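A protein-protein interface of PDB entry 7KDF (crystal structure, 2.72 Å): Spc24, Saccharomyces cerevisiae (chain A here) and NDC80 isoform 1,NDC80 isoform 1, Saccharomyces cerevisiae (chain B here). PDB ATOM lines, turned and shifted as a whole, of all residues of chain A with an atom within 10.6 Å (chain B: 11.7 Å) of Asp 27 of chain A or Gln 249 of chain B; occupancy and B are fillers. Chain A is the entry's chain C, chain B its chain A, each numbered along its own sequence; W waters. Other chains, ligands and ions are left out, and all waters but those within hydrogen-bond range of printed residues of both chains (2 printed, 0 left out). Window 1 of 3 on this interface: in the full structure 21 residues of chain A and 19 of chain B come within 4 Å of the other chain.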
ATOM      1  N   VAL A  18      13.348  14.823 -13.896  1.00  0.00           N
ATOM      2  CA  VAL A  18      12.218  14.436 -14.735  1.00  0.00           C
ATOM      3  C   VAL A  18      12.587  13.222 -15.577  1.00  0.00           C
ATOM      4  O   VAL A  18      11.796  12.283 -15.728  1.00  0.00           O
ATOM      5  CB  VAL A  18      11.782  15.620 -15.614  1.00  0.00           C
ATOM      6  CG1 VAL A  18      10.559  15.243 -16.434  1.00  0.00           C
ATOM      7  CG2 VAL A  18      11.560  16.852 -14.776  1.00  0.00           C
ATOM      8  N   GLU A  20      14.844  10.983 -14.813  1.00  0.00           N
ATOM      9  CA  GLU A  20      15.007   9.827 -13.939  1.00  0.00           C
ATOM     10  C   GLU A  20      13.678   9.322 -13.392  1.00  0.00           C
ATOM     11  O   GLU A  20      13.599   8.170 -12.953  1.00  0.00           O
ATOM     12  CB  GLU A  20      15.970  10.179 -12.805  1.00  0.00           C
ATOM     13  CG  GLU A  20      17.382  10.455 -13.306  1.00  0.00           C
ATOM     14  CD  GLU A  20      18.389  10.638 -12.190  1.00  0.00           C
ATOM     15  OE1 GLU A  20      17.986  11.042 -11.077  1.00  0.00           O
ATOM     16  OE2 GLU A  20      19.589  10.382 -12.432  1.00  0.00           O
ATOM     17  N   SER A  21      12.636  10.151 -13.416  1.00  0.00           N
ATOM     18  CA  SER A  21      11.283   9.727 -13.085  1.00  0.00           C
ATOM     19  C   SER A  21      10.513   9.230 -14.297  1.00  0.00           C
ATOM     20  O   SER A  21       9.379   8.762 -14.149  1.00  0.00           O
ATOM     21  CB  SER A  21      10.514  10.881 -12.436  1.00  0.00           C
ATOM     22  OG  SER A  21      11.278  11.464 -11.400  1.00  0.00           O
ATOM     23  N   PHE A  22      11.101   9.333 -15.488  1.00  0.00           N
ATOM     24  CA  PHE A  22      10.456   8.932 -16.734  1.00  0.00           C
ATOM     25  C   PHE A  22      10.696   7.438 -16.922  1.00  0.00           C
ATOM     26  O   PHE A  22      11.543   7.000 -17.707  1.00  0.00           O
ATOM     27  CB  PHE A  22      11.006   9.755 -17.892  1.00  0.00           C
ATOM     28  CG  PHE A  22      10.059   9.907 -19.040  1.00  0.00           C
ATOM     29  CD1 PHE A  22       9.355  11.082 -19.217  1.00  0.00           C
ATOM     30  CD2 PHE A  22       9.890   8.884 -19.958  1.00  0.00           C
ATOM     31  CE1 PHE A  22       8.493  11.234 -20.280  1.00  0.00           C
ATOM     32  CE2 PHE A  22       9.028   9.029 -21.023  1.00  0.00           C
ATOM     33  CZ  PHE A  22       8.329  10.207 -21.185  1.00  0.00           C
ATOM     34  N   ASP A  23       9.935   6.644 -16.171  1.00  0.00           N
ATOM     35  CA  ASP A  23      10.110   5.195 -16.153  1.00  0.00           C
ATOM     36  C   ASP A  23       9.635   4.605 -17.474  1.00  0.00           C
ATOM     37  O   ASP A  23       8.434   4.595 -17.762  1.00  0.00           O
ATOM     38  CB  ASP A  23       9.345   4.595 -14.979  1.00  0.00           C
ATOM     39  CG  ASP A  23       9.822   3.203 -14.618  1.00  0.00           C
ATOM     40  OD1 ASP A  23      10.357   2.498 -15.502  1.00  0.00           O
ATOM     41  OD2 ASP A  23       9.658   2.814 -13.443  1.00  0.00           O
ATOM     42  N   ILE A  24      10.570   4.104 -18.280  1.00  0.00           N
ATOM     43  CA  ILE A  24      10.202   3.530 -19.569  1.00  0.00           C
ATOM     44  C   ILE A  24       9.715   2.092 -19.404  1.00  0.00           C
ATOM     45  O   ILE A  24       8.689   1.701 -19.973  1.00  0.00           O
ATOM     46  CB  ILE A  24      11.384   3.615 -20.551  1.00  0.00           C
ATOM     47  CG1 ILE A  24      11.552   5.046 -21.059  1.00  0.00           C
ATOM     48  CG2 ILE A  24      11.180   2.664 -21.720  1.00  0.00           C
ATOM     49  CD1 ILE A  24      12.925   5.340 -21.615  1.00  0.00           C
ATOM     50  N   GLN A  25      10.440   1.287 -18.623  1.00  0.00           N
ATOM     51  CA  GLN A  25      10.121  -0.135 -18.528  1.00  0.00           C
ATOM     52  C   GLN A  25       8.724  -0.358 -17.963  1.00  0.00           C
ATOM     53  O   GLN A  25       7.998  -1.249 -18.421  1.00  0.00           O
ATOM     54  CB  GLN A  25      11.167  -0.857 -17.677  1.00  0.00           C
ATOM     55  CG  GLN A  25      11.316  -2.336 -18.011  1.00  0.00           C
ATOM     56  CD  GLN A  25      11.655  -2.580 -19.475  1.00  0.00           C
ATOM     57  OE1 GLN A  25      12.277  -1.740 -20.132  1.00  0.00           O
ATOM     58  NE2 GLN A  25      11.227  -3.726 -19.997  1.00  0.00           N
ATOM     59  N   GLN A  26       8.334   0.438 -16.966  1.00  0.00           N
ATOM     60  CA  GLN A  26       7.000   0.322 -16.387  1.00  0.00           C
ATOM     61  C   GLN A  26       5.919   0.387 -17.462  1.00  0.00           C
ATOM     62  O   GLN A  26       5.047  -0.486 -17.536  1.00  0.00           O
ATOM     63  CB  GLN A  26       6.800   1.421 -15.347  1.00  0.00           C
ATOM     64  CG  GLN A  26       5.775   1.116 -14.275  1.00  0.00           C
ATOM     65  CD  GLN A  26       5.580   2.289 -13.328  1.00  0.00           C
ATOM     66  OE1 GLN A  26       5.533   3.449 -13.750  1.00  0.00           O
ATOM     67  NE2 GLN A  26       5.466   1.993 -12.040  1.00  0.00           N
ATOM     68  N   ASP A  27       5.979   1.403 -18.326  1.00  0.00           N
ATOM     69  CA  ASP A  27       4.958   1.548 -19.360  1.00  0.00           C
ATOM     70  C   ASP A  27       5.085   0.471 -20.435  1.00  0.00           C
ATOM     71  O   ASP A  27       4.072  -0.005 -20.966  1.00  0.00           O
ATOM     72  CB  ASP A  27       5.033   2.945 -19.972  1.00  0.00           C
ATOM     73  CG  ASP A  27       4.754   4.043 -18.954  1.00  0.00           C
ATOM     74  OD1 ASP A  27       4.494   3.712 -17.779  1.00  0.00           O
ATOM     75  OD2 ASP A  27       4.792   5.236 -19.326  1.00  0.00           O
ATOM     76  N   VAL A  28       6.313   0.070 -20.773  1.00  0.00           N
ATOM     77  CA  VAL A  28       6.481  -1.008 -21.745  1.00  0.00           C
ATOM     78  C   VAL A  28       5.919  -2.309 -21.190  1.00  0.00           C
ATOM     79  O   VAL A  28       5.206  -3.046 -21.885  1.00  0.00           O
ATOM     80  CB  VAL A  28       7.962  -1.154 -22.141  1.00  0.00           C
ATOM     81  CG1 VAL A  28       8.190  -2.487 -22.844  1.00  0.00           C
ATOM     82  CG2 VAL A  28       8.386  -0.004 -23.034  1.00  0.00           C
ATOM     83  N   ASP A  29       6.221  -2.604 -19.922  1.00  0.00           N
ATOM     84  CA  ASP A  29       5.666  -3.792 -19.283  1.00  0.00           C
ATOM     85  C   ASP A  29       4.146  -3.750 -19.284  1.00  0.00           C
ATOM     86  O   ASP A  29       3.490  -4.759 -19.567  1.00  0.00           O
ATOM     87  CB  ASP A  29       6.189  -3.910 -17.853  1.00  0.00           C
ATOM     88  CG  ASP A  29       7.563  -4.537 -17.786  1.00  0.00           C
ATOM     89  OD1 ASP A  29       8.060  -5.003 -18.833  1.00  0.00           O
ATOM     90  OD2 ASP A  29       8.145  -4.565 -16.683  1.00  0.00           O
ATOM     91  N   ALA A  30       3.570  -2.586 -18.979  1.00  0.00           N
ATOM     92  CA  ALA A  30       2.124  -2.439 -19.066  1.00  0.00           C
ATOM     93  C   ALA A  30       1.622  -2.829 -20.450  1.00  0.00           C
ATOM     94  O   ALA A  30       0.633  -3.559 -20.572  1.00  0.00           O
ATOM     95  CB  ALA A  30       1.721  -1.007 -18.720  1.00  0.00           C
ATOM     96  N   MET A  31       2.322  -2.396 -21.504  1.00  0.00           N
ATOM     97  CA  MET A  31       1.888  -2.718 -22.862  1.00  0.00           C
ATOM     98  C   MET A  31       1.925  -4.217 -23.113  1.00  0.00           C
ATOM     99  O   MET A  31       1.065  -4.765 -23.816  1.00  0.00           O
ATOM    100  CB  MET A  31       2.757  -1.990 -23.886  1.00  0.00           C
ATOM    101  CG  MET A  31       2.403  -0.519 -24.052  1.00  0.00           C
ATOM    102  SD  MET A  31       0.777  -0.279 -24.801  1.00  0.00           S
ATOM    103  CE  MET A  31       0.912  -1.318 -26.251  1.00  0.00           C
ATOM    104  N   LYS A  32       2.924  -4.894 -22.551  1.00  0.00           N
ATOM    105  CA  LYS A  32       3.025  -6.342 -22.673  1.00  0.00           C
ATOM    106  C   LYS A  32       1.825  -7.036 -22.040  1.00  0.00           C
ATOM    107  O   LYS A  32       1.246  -7.960 -22.628  1.00  0.00           O
ATOM    108  CB  LYS A  32       4.331  -6.790 -22.027  1.00  0.00           C
ATOM    109  CG  LYS A  32       5.550  -6.341 -22.788  1.00  0.00           C
ATOM    110  CD  LYS A  32       6.774  -6.743 -22.044  1.00  0.00           C
ATOM    111  CE  LYS A  32       8.033  -6.292 -22.756  1.00  0.00           C
ATOM    112  NZ  LYS A  32       9.266  -6.755 -22.019  1.00  0.00           N
ATOM    113  N   ARG A  33       1.426  -6.574 -20.854  1.00  0.00           N
ATOM    114  CA  ARG A  33       0.267  -7.126 -20.165  1.00  0.00           C
ATOM    115  C   ARG A  33      -1.018  -6.847 -20.936  1.00  0.00           C
ATOM    116  O   ARG A  33      -1.896  -7.713 -21.026  1.00  0.00           O
ATOM    117  CB  ARG A  33       0.205  -6.548 -18.753  1.00  0.00           C
ATOM    118  CG  ARG A  33       1.489  -6.754 -17.957  1.00  0.00           C
ATOM    119  CD  ARG A  33       1.239  -6.622 -16.470  1.00  0.00           C
ATOM    120  NE  ARG A  33       0.702  -5.309 -16.134  1.00  0.00           N
ATOM    121  CZ  ARG A  33       1.444  -4.233 -15.892  1.00  0.00           C
ATOM    122  NH1 ARG A  33       2.765  -4.301 -15.944  1.00  0.00           N
ATOM    123  NH2 ARG A  33       0.856  -3.088 -15.600  1.00  0.00           N
ATOM    124  N   ILE A  34      -1.141  -5.646 -21.508  1.00  0.00           N
ATOM    125  CA  ILE A  34      -2.317  -5.334 -22.316  1.00  0.00           C
ATOM    126  C   ILE A  34      -2.379  -6.243 -23.536  1.00  0.00           C
ATOM    127  O   ILE A  34      -3.425  -6.827 -23.843  1.00  0.00           O
ATOM    128  CB  ILE A  34      -2.323  -3.845 -22.705  1.00  0.00           C
ATOM    129  CG1 ILE A  34      -2.276  -2.974 -21.448  1.00  0.00           C
ATOM    130  CG2 ILE A  34      -3.543  -3.524 -23.540  1.00  0.00           C
ATOM    131  CD1 ILE A  34      -2.187  -1.496 -21.737  1.00  0.00           C
ATOM    132  N   ARG A  35      -1.253  -6.405 -24.233  1.00  0.00           N
ATOM    133  CA  ARG A  35      -1.223  -7.326 -25.365  1.00  0.00           C
ATOM    134  C   ARG A  35      -1.547  -8.740 -24.918  1.00  0.00           C
ATOM    135  O   ARG A  35      -2.255  -9.477 -25.617  1.00  0.00           O
ATOM    136  CB  ARG A  35       0.143  -7.280 -26.048  1.00  0.00           C
ATOM    137  CG  ARG A  35       0.250  -8.118 -27.320  1.00  0.00           C
ATOM    138  CD  ARG A  35      -0.896  -7.854 -28.306  1.00  0.00           C
ATOM    139  NE  ARG A  35      -1.064  -6.437 -28.643  1.00  0.00           N
ATOM    140  CZ  ARG A  35      -0.146  -5.671 -29.233  1.00  0.00           C
ATOM    141  NH1 ARG A  35       1.038  -6.163 -29.582  1.00  0.00           N
ATOM    142  NH2 ARG A  35      -0.420  -4.398 -29.484  1.00  0.00           N
ATOM    143  N   ILE B 240       5.351  19.899 -19.821  1.00  0.00           N
ATOM    144  CA  ILE B 240       4.601  19.034 -20.719  1.00  0.00           C
ATOM    145  C   ILE B 240       5.214  17.643 -20.837  1.00  0.00           C
ATOM    146  O   ILE B 240       4.509  16.706 -21.235  1.00  0.00           O
ATOM    147  CB  ILE B 240       4.433  19.642 -22.125  1.00  0.00           C
ATOM    148  CG1 ILE B 240       5.712  19.512 -22.924  1.00  0.00           C
ATOM    149  CG2 ILE B 240       4.058  21.122 -22.039  1.00  0.00           C
ATOM    150  CD1 ILE B 240       5.465  19.725 -24.371  1.00  0.00           C
ATOM    151  N   THR B 241       6.502  17.480 -20.520  1.00  0.00           N
ATOM    152  CA  THR B 241       7.052  16.131 -20.425  1.00  0.00           C
ATOM    153  C   THR B 241       6.373  15.359 -19.304  1.00  0.00           C
ATOM    154  O   THR B 241       5.954  14.210 -19.486  1.00  0.00           O
ATOM    155  CB  THR B 241       8.567  16.175 -20.205  1.00  0.00           C
ATOM    156  OG1 THR B 241       9.216  16.580 -21.415  1.00  0.00           O
ATOM    157  CG2 THR B 241       9.090  14.802 -19.796  1.00  0.00           C
ATOM    158  N   SER B 242       6.241  15.987 -18.134  1.00  0.00           N
ATOM    159  CA  SER B 242       5.560  15.336 -17.022  1.00  0.00           C
ATOM    160  C   SER B 242       4.088  15.104 -17.336  1.00  0.00           C
ATOM    161  O   SER B 242       3.547  14.029 -17.049  1.00  0.00           O
ATOM    162  CB  SER B 242       5.716  16.172 -15.753  1.00  0.00           C
ATOM    163  OG  SER B 242       5.095  17.434 -15.905  1.00  0.00           O
ATOM    164  N   LYS B 243       3.421  16.100 -17.927  1.00  0.00           N
ATOM    165  CA  LYS B 243       2.017  15.923 -18.288  1.00  0.00           C
ATOM    166  C   LYS B 243       1.858  14.813 -19.318  1.00  0.00           C
ATOM    167  O   LYS B 243       0.904  14.030 -19.258  1.00  0.00           O
ATOM    168  CB  LYS B 243       1.426  17.237 -18.811  1.00  0.00           C
ATOM    169  CG  LYS B 243      -0.040  17.113 -19.203  1.00  0.00           C
ATOM    170  CD  LYS B 243      -0.712  18.449 -19.478  1.00  0.00           C
ATOM    171  CE  LYS B 243      -2.200  18.240 -19.775  1.00  0.00           C
ATOM    172  NZ  LYS B 243      -2.954  19.515 -19.954  1.00  0.00           N
ATOM    173  N   PHE B 244       2.792  14.731 -20.266  1.00  0.00           N
ATOM    174  CA  PHE B 244       2.800  13.646 -21.240  1.00  0.00           C
ATOM    175  C   PHE B 244       2.856  12.285 -20.551  1.00  0.00           C
ATOM    176  O   PHE B 244       2.011  11.415 -20.799  1.00  0.00           O
ATOM    177  CB  PHE B 244       3.990  13.852 -22.179  1.00  0.00           C
ATOM    178  CG  PHE B 244       4.281  12.708 -23.101  1.00  0.00           C
ATOM    179  CD1 PHE B 244       3.516  12.493 -24.235  1.00  0.00           C
ATOM    180  CD2 PHE B 244       5.368  11.882 -22.864  1.00  0.00           C
ATOM    181  CE1 PHE B 244       3.812  11.454 -25.097  1.00  0.00           C
ATOM    182  CE2 PHE B 244       5.669  10.842 -23.717  1.00  0.00           C
ATOM    183  CZ  PHE B 244       4.890  10.625 -24.835  1.00  0.00           C
ATOM    184  N   LYS B 245       3.827  12.095 -19.652  1.00  0.00           N
ATOM    185  CA  LYS B 245       4.041  10.781 -19.055  1.00  0.00           C
ATOM    186  C   LYS B 245       2.870  10.369 -18.178  1.00  0.00           C
ATOM    187  O   LYS B 245       2.411   9.218 -18.241  1.00  0.00           O
ATOM    188  CB  LYS B 245       5.342  10.777 -18.252  1.00  0.00           C
ATOM    189  CG  LYS B 245       5.784   9.386 -17.835  1.00  0.00           C
ATOM    190  CD  LYS B 245       5.747   8.426 -19.014  1.00  0.00           C
ATOM    191  CE  LYS B 245       6.747   7.296 -18.843  1.00  0.00           C
ATOM    192  NZ  LYS B 245       6.547   6.553 -17.571  1.00  0.00           N
ATOM    193  N   ILE B 246       2.364  11.299 -17.365  1.00  0.00           N
ATOM    194  CA  ILE B 246       1.247  10.982 -16.483  1.00  0.00           C
ATOM    195  C   ILE B 246      -0.009  10.672 -17.287  1.00  0.00           C
ATOM    196  O   ILE B 246      -0.807   9.806 -16.909  1.00  0.00           O
ATOM    197  CB  ILE B 246       1.022  12.115 -15.461  1.00  0.00           C
ATOM    198  CG1 ILE B 246       2.249  12.214 -14.550  1.00  0.00           C
ATOM    199  CG2 ILE B 246      -0.289  11.949 -14.695  1.00  0.00           C
ATOM    200  CD1 ILE B 246       2.262  13.396 -13.603  1.00  0.00           C
ATOM    201  N   ASN B 247      -0.213  11.376 -18.402  1.00  0.00           N
ATOM    202  CA  ASN B 247      -1.426  11.162 -19.187  1.00  0.00           C
ATOM    203  C   ASN B 247      -1.444   9.775 -19.816  1.00  0.00           C
ATOM    204  O   ASN B 247      -2.479   9.093 -19.797  1.00  0.00           O
ATOM    205  CB  ASN B 247      -1.561  12.247 -20.253  1.00  0.00           C
ATOM    206  CG  ASN B 247      -2.260  13.500 -19.731  1.00  0.00           C
ATOM    207  OD1 ASN B 247      -2.744  13.526 -18.598  1.00  0.00           O
ATOM    208  ND2 ASN B 247      -2.320  14.542 -20.559  1.00  0.00           N
ATOM    209  N   ILE B 248      -0.311   9.338 -20.374  1.00  0.00           N
ATOM    210  CA  ILE B 248      -0.241   7.994 -20.940  1.00  0.00           C
ATOM    211  C   ILE B 248      -0.293   6.943 -19.845  1.00  0.00           C
ATOM    212  O   ILE B 248      -0.852   5.856 -20.037  1.00  0.00           O
ATOM    213  CB  ILE B 248       1.001   7.832 -21.837  1.00  0.00           C
ATOM    214  CG1 ILE B 248       0.855   8.762 -23.039  1.00  0.00           C
ATOM    215  CG2 ILE B 248       1.243   6.365 -22.217  1.00  0.00           C
ATOM    216  CD1 ILE B 248       2.058   8.847 -23.910  1.00  0.00           C
ATOM    217  N   GLN B 249       0.306   7.231 -18.687  1.00  0.00           N
ATOM    218  CA  GLN B 249       0.161   6.319 -17.561  1.00  0.00           C
ATOM    219  C   GLN B 249      -1.308   6.111 -17.222  1.00  0.00           C
ATOM    220  O   GLN B 249      -1.729   4.990 -16.911  1.00  0.00           O
ATOM    221  CB  GLN B 249       0.928   6.840 -16.349  1.00  0.00           C
ATOM    222  CG  GLN B 249       2.367   6.368 -16.310  1.00  0.00           C
ATOM    223  CD  GLN B 249       3.122   6.896 -15.111  1.00  0.00           C
ATOM    224  OE1 GLN B 249       2.875   8.013 -14.654  1.00  0.00           O
ATOM    225  NE2 GLN B 249       4.065   6.103 -14.605  1.00  0.00           N
ATOM    226  N   SER B 250      -2.105   7.179 -17.295  1.00  0.00           N
ATOM    227  CA  SER B 250      -3.543   7.052 -17.093  1.00  0.00           C
ATOM    228  C   SER B 250      -4.181   6.183 -18.172  1.00  0.00           C
ATOM    229  O   SER B 250      -5.031   5.334 -17.873  1.00  0.00           O
ATOM    230  CB  SER B 250      -4.184   8.440 -17.067  1.00  0.00           C
ATOM    231  OG  SER B 250      -5.598   8.357 -17.058  1.00  0.00           O
ATOM    232  N   SER B 251      -3.789   6.378 -19.432  1.00  0.00           N
ATOM    233  CA  SER B 251      -4.368   5.580 -20.508  1.00  0.00           C
ATOM    234  C   SER B 251      -4.047   4.103 -20.329  1.00  0.00           C
ATOM    235  O   SER B 251      -4.921   3.243 -20.500  1.00  0.00           O
ATOM    236  CB  SER B 251      -3.864   6.074 -21.864  1.00  0.00           C
ATOM    237  OG  SER B 251      -4.533   7.261 -22.254  1.00  0.00           O
ATOM    238  N   LEU B 252      -2.797   3.794 -19.975  1.00  0.00           N
ATOM    239  CA  LEU B 252      -2.399   2.409 -19.755  1.00  0.00           C
ATOM    240  C   LEU B 252      -3.170   1.794 -18.596  1.00  0.00           C
ATOM    241  O   LEU B 252      -3.615   0.642 -18.674  1.00  0.00           O
ATOM    242  CB  LEU B 252      -0.894   2.344 -19.496  1.00  0.00           C
ATOM    243  CG  LEU B 252       0.035   2.642 -20.674  1.00  0.00           C
ATOM    244  CD1 LEU B 252       1.464   2.781 -20.187  1.00  0.00           C
ATOM    245  CD2 LEU B 252      -0.061   1.564 -21.748  1.00  0.00           C
ATOM    246  N   GLU B 253      -3.339   2.551 -17.509  1.00  0.00           N
ATOM    247  CA  GLU B 253      -4.045   2.049 -16.335  1.00  0.00           C
ATOM    248  C   GLU B 253      -5.514   1.778 -16.637  1.00  0.00           C
ATOM    249  O   GLU B 253      -6.061   0.754 -16.214  1.00  0.00           O
ATOM    250  CB  GLU B 253      -3.898   3.049 -15.191  1.00  0.00           C
ATOM    251  CG  GLU B 253      -4.274   2.530 -13.816  1.00  0.00           C
ATOM    252  CD  GLU B 253      -4.364   3.655 -12.792  1.00  0.00           C
ATOM    253  OE1 GLU B 253      -4.303   4.837 -13.198  1.00  0.00           O
ATOM    254  OE2 GLU B 253      -4.492   3.358 -11.585  1.00  0.00           O
ATOM    255  N   ASN B 254      -6.171   2.685 -17.363  1.00  0.00           N
ATOM    256  CA  ASN B 254      -7.584   2.498 -17.669  1.00  0.00           C
ATOM    257  C   ASN B 254      -7.804   1.284 -18.562  1.00  0.00           C
ATOM    258  O   ASN B 254      -8.747   0.513 -18.350  1.00  0.00           O
ATOM    259  CB  ASN B 254      -8.149   3.758 -18.322  1.00  0.00           C
ATOM    260  CG  ASN B 254      -8.413   4.861 -17.318  1.00  0.00           C
ATOM    261  OD1 ASN B 254      -8.543   4.605 -16.121  1.00  0.00           O
ATOM    262  ND2 ASN B 254      -8.485   6.098 -17.798  1.00  0.00           N
ATOM    263  N   SER B 255      -6.943   1.095 -19.564  1.00  0.00           N
ATOM    264  CA  SER B 255      -7.114  -0.027 -20.481  1.00  0.00           C
ATOM    265  C   SER B 255      -6.987  -1.360 -19.754  1.00  0.00           C
ATOM    266  O   SER B 255      -7.754  -2.296 -20.015  1.00  0.00           O
ATOM    267  CB  SER B 255      -6.094   0.069 -21.615  1.00  0.00           C
ATOM    268  OG  SER B 255      -6.142  -1.082 -22.441  1.00  0.00           O
ATOM    269  N   GLU B 256      -6.019  -1.463 -18.839  1.00  0.00           N
ATOM    270  CA  GLU B 256      -5.758  -2.729 -18.162  1.00  0.00           C
ATOM    271  C   GLU B 256      -6.917  -3.140 -17.257  1.00  0.00           C
ATOM    272  O   GLU B 256      -7.330  -4.311 -17.279  1.00  0.00           O
ATOM    273  CB  GLU B 256      -4.443  -2.628 -17.388  1.00  0.00           C
ATOM    274  CG  GLU B 256      -3.741  -3.953 -17.187  1.00  0.00           C
ATOM    275  CD  GLU B 256      -2.347  -3.807 -16.615  1.00  0.00           C
ATOM    276  OE1 GLU B 256      -1.968  -2.682 -16.225  1.00  0.00           O
ATOM    277  OE2 GLU B 256      -1.639  -4.833 -16.527  1.00  0.00           O
ATOM    278  N   ASN B 257      -7.456  -2.196 -16.462  1.00  0.00           N
ATOM    279  CA  ASN B 257      -8.692  -2.463 -15.731  1.00  0.00           C
ATOM    280  C   ASN B 257      -9.865  -2.753 -16.660  1.00  0.00           C
ATOM    281  O   ASN B 257     -10.703  -3.601 -16.333  1.00  0.00           O
ATOM    282  CB  ASN B 257      -9.033  -1.326 -14.770  1.00  0.00           C
ATOM    283  CG  ASN B 257      -8.102  -1.260 -13.575  1.00  0.00           C
ATOM    284  OD1 ASN B 257      -7.323  -0.319 -13.407  1.00  0.00           O
ATOM    285  ND2 ASN B 257      -8.278  -2.223 -12.662  1.00  0.00           N
ATOM    286  N   GLU B 258      -9.964  -2.066 -17.804  1.00  0.00           N
ATOM    287  CA  GLU B 258     -11.036  -2.389 -18.734  1.00  0.00           C
ATOM    288  C   GLU B 258     -10.964  -3.852 -19.135  1.00  0.00           C
ATOM    289  O   GLU B 258     -11.948  -4.588 -19.018  1.00  0.00           O
ATOM    290  CB  GLU B 258     -10.960  -1.485 -19.962  1.00  0.00           C
ATOM    291  CG  GLU B 258     -11.637  -0.144 -19.798  1.00  0.00           C
ATOM    292  CD  GLU B 258     -11.105   0.887 -20.770  1.00  0.00           C
ATOM    293  OE1 GLU B 258     -11.055   2.077 -20.395  1.00  0.00           O
ATOM    294  OE2 GLU B 258     -10.712   0.506 -21.893  1.00  0.00           O
HETATM  295  O   HOH W   1       7.273   7.508 -15.021  1.00  0.00           O
HETATM  296  O   HOH W   2       6.201   6.276 -12.884  1.00  0.00           O
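Water W1 lies within hydrogen-bond range of the backbone carbonyl oxygen (O) of Ser 21 of chain A (2.6 Å), the side-chain amino group (NZ) of Lys 245 of chain B (2.8 Å) and the backbone NH (N) of Asp 23 of chain A (3.0 Å).
Water W2 lies within hydrogen-bond range of NE2 of Gln 249 of chain B (2.7 Å) and OE1 of Gln 26 of chain A (3.0 Å).
N of Gln 25 of chain A lies within hydrogen-bond range of OD1 of Asp 23 of chain A (3.3 Å).
The backbone NH (N) of Gln 26 of chain A sits at hydrogen-bond distance from the side-chain carboxylate (OD1) of Asp 23 of chain A (3.2 Å).
Of chain B, only Lys 245 (2.8 Å), Gln 249 (3.7 Å) and Leu 252 (3.6 Å) come within 4 Å of Asp 27 of chain A.
Gln 249 of chain B touches two residues of chain A.
Asp 23 of chain A touches just one residue of chain B: Lys 245.
No residue of chain B comes within 4 Å of Gln 25 of chain A.
No residue of chain B comes within 4 Å of Val 28 of chain A.
No residue of chain B comes within 4 Å of Asp 29 of chain A.
No residue of chain B comes within 4 Å of Ala 30 of chain A.
Lys 245 of chain B touches just these residues of chain A: Phe 22 (3.6 Å), Asp 23 (2.7 Å) and Asp 27 (2.8 Å).
Ile 248 of chain B touches none of the printed residues of chain A.
No residue of chain A comes within 4 Å of Ser 250 of chain B.
Ser 251 of chain B touches none of the printed residues of chain A.
Leu 252 of chain B touches three residues of chain A.
No residue of chain A comes within 4 Å of Glu 253 of chain B.
Printed residues of chain A within 4 Å of Phe 244 of chain B: Phe 22.
Of the printed residues of chain B, Arg 33 of chain A touches Glu 256 (2.4 Å).
Ile 24 of chain A touches none of the printed residues of chain B.
The nearest residue of chain B that does not touch Asp 27 of chain A is Ile 248 of chain B (4.7 Å).
The nearest printed residue of chain B that does not touch Val 18 of chain A is Ser 242 of chain B (4.7 Å).
Among the printed residues, pairs that only touch across the chains: Asp 27 of chain A with Leu 252 of chain B (3.6 Å), Phe 22 of chain A with Lys 245 of chain B (3.6 Å), Phe 22 of chain A with Thr 241 of chain B (3.6 Å), Met 31 of chain A with Leu 252 of chain B (3.7 Å), Val 18 of chain A with Thr 241 of chain B (3.7 Å), Asp 27 of chain A with Gln 249 of chain B (3.7 Å), Ile 34 of chain A with Leu 252 of chain B (3.7 Å), Phe 22 of chain A with Phe 244 of chain B (3.7 Å) and Ile 34 of chain A with Ser 255 of chain B (3.7 Å).
The side-chain amino group (NZ) of Lys 245 of chain B is in salt-bridge range of the side-chain carboxylate (OD2) of Asp 27 of chain A (2.8 Å).
The side-chain amide nitrogen (NE2) of Gln 249 of chain B lies within hydrogen-bond range of the side-chain amide oxygen (OE1) of Gln 26 of chain A (3.2 Å).
The guanidinium group of Arg 33 of chain A is in salt-bridge range of the side-chain carboxylate of Glu 256 of chain B, 2.4 Å away.
The backbone carbonyl oxygen (O) of Asp 23 of chain A is in hydrogen-bond range of the side-chain amino group (NZ) of Lys 245 of chain B (2.7 Å).
Hydrophobic or aromatic side chains of chain A within 4 Å of the printed part of chain B: Val 18, Phe 22, Met 31 and Ile 34.
Of the 19 printed residues of chain B, 7 touch a printed residue of chain A.
Printed residues of chain B that touch a printed residue of chain A: Thr 241, Phe 244, Lys 245, Gln 249, Leu 252, Ser 255 and Glu 256.
Hydrophobic or aromatic side chains of chain B within 4 Å of the printed part of chain A: Phe 244 and Leu 252.
Among the printed residues, 13 pairs touch across the chains.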
